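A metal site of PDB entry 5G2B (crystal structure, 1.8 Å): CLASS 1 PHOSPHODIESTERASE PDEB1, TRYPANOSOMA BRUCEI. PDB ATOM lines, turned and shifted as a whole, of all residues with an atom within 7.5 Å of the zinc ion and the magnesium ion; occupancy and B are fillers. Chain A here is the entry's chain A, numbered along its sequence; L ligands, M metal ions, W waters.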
ATOM      1  N   TYR A 110      16.711   6.070  32.796  1.00  0.00           N
ATOM      2  CA  TYR A 110      16.573   6.726  31.506  1.00  0.00           C
ATOM      3  C   TYR A 110      17.615   7.836  31.248  1.00  0.00           C
ATOM      4  O   TYR A 110      18.355   7.741  30.268  1.00  0.00           O
ATOM      5  CB  TYR A 110      15.150   7.238  31.264  1.00  0.00           C
ATOM      6  CG  TYR A 110      14.970   7.795  29.869  1.00  0.00           C
ATOM      7  CD1 TYR A 110      14.711   6.955  28.795  1.00  0.00           C
ATOM      8  CD2 TYR A 110      15.053   9.159  29.623  1.00  0.00           C
ATOM      9  CE1 TYR A 110      14.527   7.450  27.513  1.00  0.00           C
ATOM     10  CE2 TYR A 110      14.868   9.679  28.337  1.00  0.00           C
ATOM     11  CZ  TYR A 110      14.612   8.811  27.294  1.00  0.00           C
ATOM     12  OH  TYR A 110      14.451   9.306  26.047  1.00  0.00           O
ATOM     13  N   HIS A 111      17.703   8.885  32.094  1.00  0.00           N
ATOM     14  CA  HIS A 111      18.626  10.004  31.807  1.00  0.00           C
ATOM     15  C   HIS A 111      20.017   9.728  32.325  1.00  0.00           C
ATOM     16  O   HIS A 111      20.589  10.464  33.129  1.00  0.00           O
ATOM     17  CB  HIS A 111      18.114  11.347  32.347  1.00  0.00           C
ATOM     18  CG  HIS A 111      16.847  11.815  31.708  1.00  0.00           C
ATOM     19  ND1 HIS A 111      15.629  11.681  32.312  1.00  0.00           N
ATOM     20  CD2 HIS A 111      16.613  12.430  30.530  1.00  0.00           C
ATOM     21  CE1 HIS A 111      14.687  12.196  31.537  1.00  0.00           C
ATOM     22  NE2 HIS A 111      15.261  12.652  30.439  1.00  0.00           N
ATOM     23  N   HIS A 115      21.482   7.474  27.185  1.00  0.00           N
ATOM     24  CA  HIS A 115      20.529   8.375  26.548  1.00  0.00           C
ATOM     25  C   HIS A 115      21.202   9.461  25.703  1.00  0.00           C
ATOM     26  O   HIS A 115      20.695   9.805  24.600  1.00  0.00           O
ATOM     27  CB  HIS A 115      19.701   9.037  27.594  1.00  0.00           C
ATOM     28  CG  HIS A 115      18.857  10.163  27.084  1.00  0.00           C
ATOM     29  ND1 HIS A 115      17.933  10.003  26.094  1.00  0.00           N
ATOM     30  CD2 HIS A 115      18.830  11.461  27.411  1.00  0.00           C
ATOM     31  CE1 HIS A 115      17.322  11.146  25.868  1.00  0.00           C
ATOM     32  NE2 HIS A 115      17.827  12.038  26.697  1.00  0.00           N
ATOM     33  N   VAL A 116      22.245  10.063  26.233  1.00  0.00           N
ATOM     34  CA  VAL A 116      22.908  11.156  25.518  1.00  0.00           C
ATOM     35  C   VAL A 116      23.746  10.666  24.316  1.00  0.00           C
ATOM     36  O   VAL A 116      23.837  11.332  23.288  1.00  0.00           O
ATOM     37  CB  VAL A 116      23.699  12.104  26.478  1.00  0.00           C
ATOM     38  CG1 VAL A 116      22.874  12.573  27.648  1.00  0.00           C
ATOM     39  CG2 VAL A 116      24.980  11.504  26.956  1.00  0.00           C
ATOM     40  N   VAL A 119      21.149  10.099  21.749  1.00  0.00           N
ATOM     41  CA  VAL A 119      20.761  11.402  21.136  1.00  0.00           C
ATOM     42  C   VAL A 119      21.820  11.875  20.112  1.00  0.00           C
ATOM     43  O   VAL A 119      21.453  12.293  19.056  1.00  0.00           O
ATOM     44  CB  VAL A 119      20.450  12.508  22.185  1.00  0.00           C
ATOM     45  CG1 VAL A 119      20.182  13.888  21.484  1.00  0.00           C
ATOM     46  CG2 VAL A 119      19.212  12.075  23.036  1.00  0.00           C
ATOM     47  N   ALA A 148      24.781  17.203  22.147  1.00  0.00           N
ATOM     48  CA  ALA A 148      24.081  15.995  22.519  1.00  0.00           C
ATOM     49  C   ALA A 148      24.600  15.338  23.815  1.00  0.00           C
ATOM     50  O   ALA A 148      23.804  14.845  24.646  1.00  0.00           O
ATOM     51  CB  ALA A 148      24.133  15.002  21.368  1.00  0.00           C
ATOM     52  N   HIS A 151      23.746  17.430  27.200  1.00  0.00           N
ATOM     53  CA  HIS A 151      22.499  18.073  27.347  1.00  0.00           C
ATOM     54  C   HIS A 151      21.665  17.640  28.538  1.00  0.00           C
ATOM     55  O   HIS A 151      20.692  18.280  28.824  1.00  0.00           O
ATOM     56  CB  HIS A 151      21.676  17.996  26.058  1.00  0.00           C
ATOM     57  CG  HIS A 151      20.836  16.780  25.964  1.00  0.00           C
ATOM     58  ND1 HIS A 151      21.314  15.591  25.475  1.00  0.00           N
ATOM     59  CD2 HIS A 151      19.586  16.534  26.376  1.00  0.00           C
ATOM     60  CE1 HIS A 151      20.388  14.669  25.560  1.00  0.00           C
ATOM     61  NE2 HIS A 151      19.314  15.231  26.068  1.00  0.00           N
ATOM     62  N   ASP A 152      21.992  16.521  29.172  1.00  0.00           N
ATOM     63  CA  ASP A 152      21.286  16.104  30.417  1.00  0.00           C
ATOM     64  C   ASP A 152      22.284  15.867  31.578  1.00  0.00           C
ATOM     65  O   ASP A 152      22.005  15.114  32.509  1.00  0.00           O
ATOM     66  CB  ASP A 152      20.456  14.838  30.208  1.00  0.00           C
ATOM     67  CG  ASP A 152      19.110  15.103  29.566  1.00  0.00           C
ATOM     68  OD1 ASP A 152      18.400  16.129  29.814  1.00  0.00           O
ATOM     69  OD2 ASP A 152      18.806  14.289  28.682  1.00  0.00           O
ATOM     70  N   LEU A 153      23.423  16.517  31.539  1.00  0.00           N
ATOM     71  CA  LEU A 153      24.478  16.272  32.540  1.00  0.00           C
ATOM     72  C   LEU A 153      23.935  16.340  33.993  1.00  0.00           C
ATOM     73  O   LEU A 153      23.252  17.272  34.349  1.00  0.00           O
ATOM     74  CB  LEU A 153      25.619  17.284  32.422  1.00  0.00           C
ATOM     75  CG  LEU A 153      26.583  17.113  31.243  1.00  0.00           C
ATOM     76  CD1 LEU A 153      27.272  18.447  31.074  1.00  0.00           C
ATOM     77  CD2 LEU A 153      27.588  15.972  31.403  1.00  0.00           C
ATOM     78  N   HIS A 155      21.699  14.575  35.512  1.00  0.00           N
ATOM     79  CA  HIS A 155      20.290  14.441  35.675  1.00  0.00           C
ATOM     80  C   HIS A 155      20.073  13.392  36.770  1.00  0.00           C
ATOM     81  O   HIS A 155      20.787  12.401  36.791  1.00  0.00           O
ATOM     82  CB  HIS A 155      19.673  13.993  34.355  1.00  0.00           C
ATOM     83  CG  HIS A 155      18.210  14.225  34.263  1.00  0.00           C
ATOM     84  ND1 HIS A 155      17.310  13.517  35.012  1.00  0.00           N
ATOM     85  CD2 HIS A 155      17.491  15.034  33.454  1.00  0.00           C
ATOM     86  CE1 HIS A 155      16.078  13.903  34.703  1.00  0.00           C
ATOM     87  NE2 HIS A 155      16.160  14.816  33.752  1.00  0.00           N
ATOM     88  N   LEU A 183      16.592  22.067  35.448  1.00  0.00           N
ATOM     89  CA  LEU A 183      17.615  21.108  35.060  1.00  0.00           C
ATOM     90  C   LEU A 183      18.481  21.661  33.906  1.00  0.00           C
ATOM     91  O   LEU A 183      19.673  21.445  33.890  1.00  0.00           O
ATOM     92  CB  LEU A 183      17.043  19.769  34.652  1.00  0.00           C
ATOM     93  CG  LEU A 183      16.455  18.995  35.822  1.00  0.00           C
ATOM     94  CD1 LEU A 183      15.395  17.981  35.372  1.00  0.00           C
ATOM     95  CD2 LEU A 183      17.572  18.336  36.635  1.00  0.00           C
ATOM     96  N   GLU A 184      17.865  22.361  32.970  1.00  0.00           N
ATOM     97  CA  GLU A 184      18.594  22.737  31.747  1.00  0.00           C
ATOM     98  C   GLU A 184      19.691  23.738  32.058  1.00  0.00           C
ATOM     99  O   GLU A 184      20.817  23.645  31.548  1.00  0.00           O
ATOM    100  CB  GLU A 184      17.624  23.221  30.654  1.00  0.00           C
ATOM    101  CG  GLU A 184      16.692  22.068  30.144  1.00  0.00           C
ATOM    102  CD  GLU A 184      15.567  21.636  31.090  1.00  0.00           C
ATOM    103  OE1 GLU A 184      15.220  22.369  32.062  1.00  0.00           O
ATOM    104  OE2 GLU A 184      15.039  20.507  30.881  1.00  0.00           O
ATOM    105  N   HIS A 187      22.492  21.695  33.526  1.00  0.00           N
ATOM    106  CA  HIS A 187      23.292  20.998  32.540  1.00  0.00           C
ATOM    107  C   HIS A 187      24.209  21.991  31.879  1.00  0.00           C
ATOM    108  O   HIS A 187      25.354  21.687  31.674  1.00  0.00           O
ATOM    109  CB  HIS A 187      22.468  20.276  31.448  1.00  0.00           C
ATOM    110  CG  HIS A 187      21.309  19.491  31.940  1.00  0.00           C
ATOM    111  ND1 HIS A 187      21.380  18.624  33.012  1.00  0.00           N
ATOM    112  CD2 HIS A 187      20.036  19.419  31.492  1.00  0.00           C
ATOM    113  CE1 HIS A 187      20.217  18.045  33.183  1.00  0.00           C
ATOM    114  NE2 HIS A 187      19.375  18.516  32.276  1.00  0.00           N
ATOM    115  N   VAL A 222      20.425  23.460  24.632  1.00  0.00           N
ATOM    116  CA  VAL A 222      20.137  22.745  25.862  1.00  0.00           C
ATOM    117  C   VAL A 222      18.952  23.405  26.538  1.00  0.00           C
ATOM    118  O   VAL A 222      18.034  22.726  26.998  1.00  0.00           O
ATOM    119  CB  VAL A 222      21.370  22.691  26.838  1.00  0.00           C
ATOM    120  CG1 VAL A 222      20.984  22.056  28.189  1.00  0.00           C
ATOM    121  CG2 VAL A 222      22.513  21.962  26.176  1.00  0.00           C
ATOM    122  N   THR A 225      15.569  22.262  25.197  1.00  0.00           N
ATOM    123  CA  THR A 225      15.057  20.937  25.446  1.00  0.00           C
ATOM    124  C   THR A 225      14.070  20.890  26.603  1.00  0.00           C
ATOM    125  O   THR A 225      13.494  19.796  26.828  1.00  0.00           O
ATOM    126  CB  THR A 225      16.169  19.919  25.796  1.00  0.00           C
ATOM    127  OG1 THR A 225      16.894  20.351  26.945  1.00  0.00           O
ATOM    128  CG2 THR A 225      17.101  19.822  24.657  1.00  0.00           C
ATOM    129  N   ASP A 226      13.868  21.987  27.339  1.00  0.00           N
ATOM    130  CA  ASP A 226      12.825  22.003  28.371  1.00  0.00           C
ATOM    131  C   ASP A 226      11.477  21.817  27.689  1.00  0.00           C
ATOM    132  O   ASP A 226      11.008  22.707  26.980  1.00  0.00           O
ATOM    133  CB  ASP A 226      12.774  23.316  29.130  1.00  0.00           C
ATOM    134  CG  ASP A 226      11.727  23.314  30.260  1.00  0.00           C
ATOM    135  OD1 ASP A 226      10.843  22.462  30.318  1.00  0.00           O
ATOM    136  OD2 ASP A 226      11.842  24.199  31.097  1.00  0.00           O
ATOM    137  N   MET A 227      10.813  20.713  27.960  1.00  0.00           N
ATOM    138  CA  MET A 227       9.523  20.427  27.290  1.00  0.00           C
ATOM    139  C   MET A 227       8.424  21.418  27.614  1.00  0.00           C
ATOM    140  O   MET A 227       7.419  21.480  26.901  1.00  0.00           O
ATOM    141  CB  MET A 227       9.051  18.955  27.510  1.00  0.00           C
ATOM    142  CG  MET A 227       9.859  17.934  26.722  1.00  0.00           C
ATOM    143  SD  MET A 227       9.793  18.201  24.919  1.00  0.00           S
ATOM    144  CE  MET A 227       8.259  17.357  24.569  1.00  0.00           C
ATOM    145  N   LEU A 260      18.073  19.157  18.140  1.00  0.00           N
ATOM    146  CA  LEU A 260      18.347  18.565  19.420  1.00  0.00           C
ATOM    147  C   LEU A 260      17.028  18.127  20.052  1.00  0.00           C
ATOM    148  O   LEU A 260      16.973  17.052  20.615  1.00  0.00           O
ATOM    149  CB  LEU A 260      19.173  19.494  20.368  1.00  0.00           C
ATOM    150  CG  LEU A 260      19.381  18.929  21.754  1.00  0.00           C
ATOM    151  CD1 LEU A 260      20.303  17.698  21.811  1.00  0.00           C
ATOM    152  CD2 LEU A 260      19.965  19.997  22.653  1.00  0.00           C
ATOM    153  N   GLY A 263      16.071  14.759  18.449  1.00  0.00           N
ATOM    154  CA  GLY A 263      16.872  13.720  19.088  1.00  0.00           C
ATOM    155  C   GLY A 263      16.271  13.277  20.417  1.00  0.00           C
ATOM    156  O   GLY A 263      16.196  12.071  20.742  1.00  0.00           O
ATOM    157  N   ASP A 264      15.856  14.240  21.201  1.00  0.00           N
ATOM    158  CA  ASP A 264      15.397  13.968  22.555  1.00  0.00           C
ATOM    159  C   ASP A 264      14.039  13.296  22.593  1.00  0.00           C
ATOM    160  O   ASP A 264      13.747  12.624  23.543  1.00  0.00           O
ATOM    161  CB  ASP A 264      15.303  15.316  23.300  1.00  0.00           C
ATOM    162  CG  ASP A 264      15.744  15.264  24.717  1.00  0.00           C
ATOM    163  OD1 ASP A 264      16.504  14.350  25.146  1.00  0.00           O
ATOM    164  OD2 ASP A 264      15.355  16.270  25.384  1.00  0.00           O
ATOM    165  N   ILE A 265      13.171  13.478  21.583  1.00  0.00           N
ATOM    166  CA  ILE A 265      11.932  12.707  21.545  1.00  0.00           C
ATOM    167  C   ILE A 265      11.905  11.689  20.415  1.00  0.00           C
ATOM    168  O   ILE A 265      10.837  11.327  19.947  1.00  0.00           O
ATOM    169  CB  ILE A 265      10.659  13.609  21.429  1.00  0.00           C
ATOM    170  CG1 ILE A 265      10.753  14.555  20.261  1.00  0.00           C
ATOM    171  CG2 ILE A 265      10.416  14.382  22.730  1.00  0.00           C
ATOM    172  CD1 ILE A 265       9.491  15.345  20.058  1.00  0.00           C
HETATM  173  C1  LIG L   1       9.258   6.936  25.002  1.00  0.00           C
HETATM  174  N1  LIG L   1       3.387   6.614  31.143  1.00  0.00           N
HETATM  175  O1  LIG L   1       8.280   7.676  25.737  1.00  0.00           O
HETATM  176  C2  LIG L   1       8.643   8.914  26.212  1.00  0.00           C
HETATM  177  N2  LIG L   1       2.312   3.408  32.424  1.00  0.00           N
HETATM  178  O2  LIG L   1       2.190   6.980  29.280  1.00  0.00           O
HETATM  179  C3  LIG L   1       9.744   9.635  25.749  1.00  0.00           C
HETATM  180  N3  LIG L   1       8.489  13.337  28.420  1.00  0.00           N
HETATM  181  O3  LIG L   1       2.752   3.881  30.270  1.00  0.00           O
HETATM  182  C4  LIG L   1      10.053  10.859  26.324  1.00  0.00           C
HETATM  183  N4  LIG L   1       8.634  14.653  28.843  1.00  0.00           N
HETATM  184  O4  LIG L   1       9.972  16.411  29.496  1.00  0.00           O
HETATM  185  C5  LIG L   1       9.263  11.397  27.352  1.00  0.00           C
HETATM  186  C6  LIG L   1       8.176  10.651  27.811  1.00  0.00           C
HETATM  187  C7  LIG L   1       7.850   9.413  27.263  1.00  0.00           C
HETATM  188  C8  LIG L   1       6.721   8.650  27.879  1.00  0.00           C
HETATM  189  C9  LIG L   1       6.779   8.288  29.213  1.00  0.00           C
HETATM  190  C10 LIG L   1       5.690   7.711  29.852  1.00  0.00           C
HETATM  191  C11 LIG L   1       4.506   7.482  29.164  1.00  0.00           C
HETATM  192  C12 LIG L   1       4.448   7.807  27.804  1.00  0.00           C
HETATM  193  C13 LIG L   1       5.545   8.387  27.179  1.00  0.00           C
HETATM  194  C14 LIG L   1       3.267   6.982  29.856  1.00  0.00           C
HETATM  195  C15 LIG L   1       2.437   5.721  31.777  1.00  0.00           C
HETATM  196  C16 LIG L   1       2.521   4.246  31.422  1.00  0.00           C
HETATM  197  C17 LIG L   1       9.508  12.753  27.890  1.00  0.00           C
HETATM  198  C18 LIG L   1       7.296  15.259  28.889  1.00  0.00           C
HETATM  199  C19 LIG L   1       6.670  15.293  27.420  1.00  0.00           C
HETATM  200  C20 LIG L   1       5.189  15.623  27.221  1.00  0.00           C
HETATM  201  C21 LIG L   1       4.211  14.750  27.994  1.00  0.00           C
HETATM  202  C22 LIG L   1       3.930  15.181  29.435  1.00  0.00           C
HETATM  203  C23 LIG L   1       5.095  15.264  30.447  1.00  0.00           C
HETATM  204  C24 LIG L   1       6.412  14.577  30.055  1.00  0.00           C
HETATM  205  C25 LIG L   1       9.837  15.251  29.165  1.00  0.00           C
HETATM  206  C26 LIG L   1      11.050  14.349  29.006  1.00  0.00           C
HETATM  207  C27 LIG L   1      12.425  15.033  28.955  1.00  0.00           C
HETATM  208  C28 LIG L   1      12.706  15.630  27.610  1.00  0.00           C
HETATM  209  C29 LIG L   1      12.070  15.262  26.494  1.00  0.00           C
HETATM  210  C30 LIG L   1      10.899  14.310  26.486  1.00  0.00           C
HETATM  211  C31 LIG L   1      10.851  13.456  27.764  1.00  0.00           C
HETATM  212 ZN    ZN M   1      17.526  14.307  26.982  1.00  0.00          ZN
HETATM  213 MG    MG M   2      16.780  17.105  29.459  1.00  0.00          MG
HETATM  214  O   HOH W   1      15.574  15.674  30.144  1.00  0.00           O
HETATM  215  O   HOH W   2      15.162  18.397  29.103  1.00  0.00           O
HETATM  216  O   HOH W   3      16.616  16.268  27.630  1.00  0.00           O
HETATM  217  O   HOH W   4      17.831  18.639  28.858  1.00  0.00           O
HETATM  218  O   HOH W   5      16.733  17.915  31.456  1.00  0.00           O
HETATM  219  O   HOH W   6      15.508  13.665  27.823  1.00  0.00           O
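O of Ala 148 lies within hydrogen-bond range of ND1 of His 151, 2.7 Å away.
The magnesium ion is bound by the side-chain carboxylate (OD1) of Asp 152 (1.9 Å).
Water W4 binds the magnesium ion, at 2.0 Å.
Water W1 is bound to the magnesium ion, at 2.0 Å.
Water W3 binds the magnesium ion, at 2.0 Å.
Water W2 binds the magnesium ion (2.1 Å).
Water W5 is bound to the magnesium ion (2.2 Å).
The magnesium ion has six donor atoms within binding distance.
Within 4 Å of the magnesium ion: Asp 152.
Water W4 bridges the side-chain hydroxyl of Thr 225 and the backbone carbonyl oxygen of His 151.
Water W5 lies within hydrogen-bond range of NE2 of His 187 (2.8 Å) and OE2 of Glu 184 (3.1 Å).
Water W2 bridges OE2 of Glu 184 and O of Thr 225.
The zinc ion is bound by OD1 of Asp 264 (2.1 Å), OD2 of Asp 152 (2.1 Å), NE2 of His 151 (2.2 Å), water W3 (2.3 Å), water W6 (2.3 Å) and NE2 of His 115 (2.3 Å).
The zinc ion has six donor atoms within binding distance.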
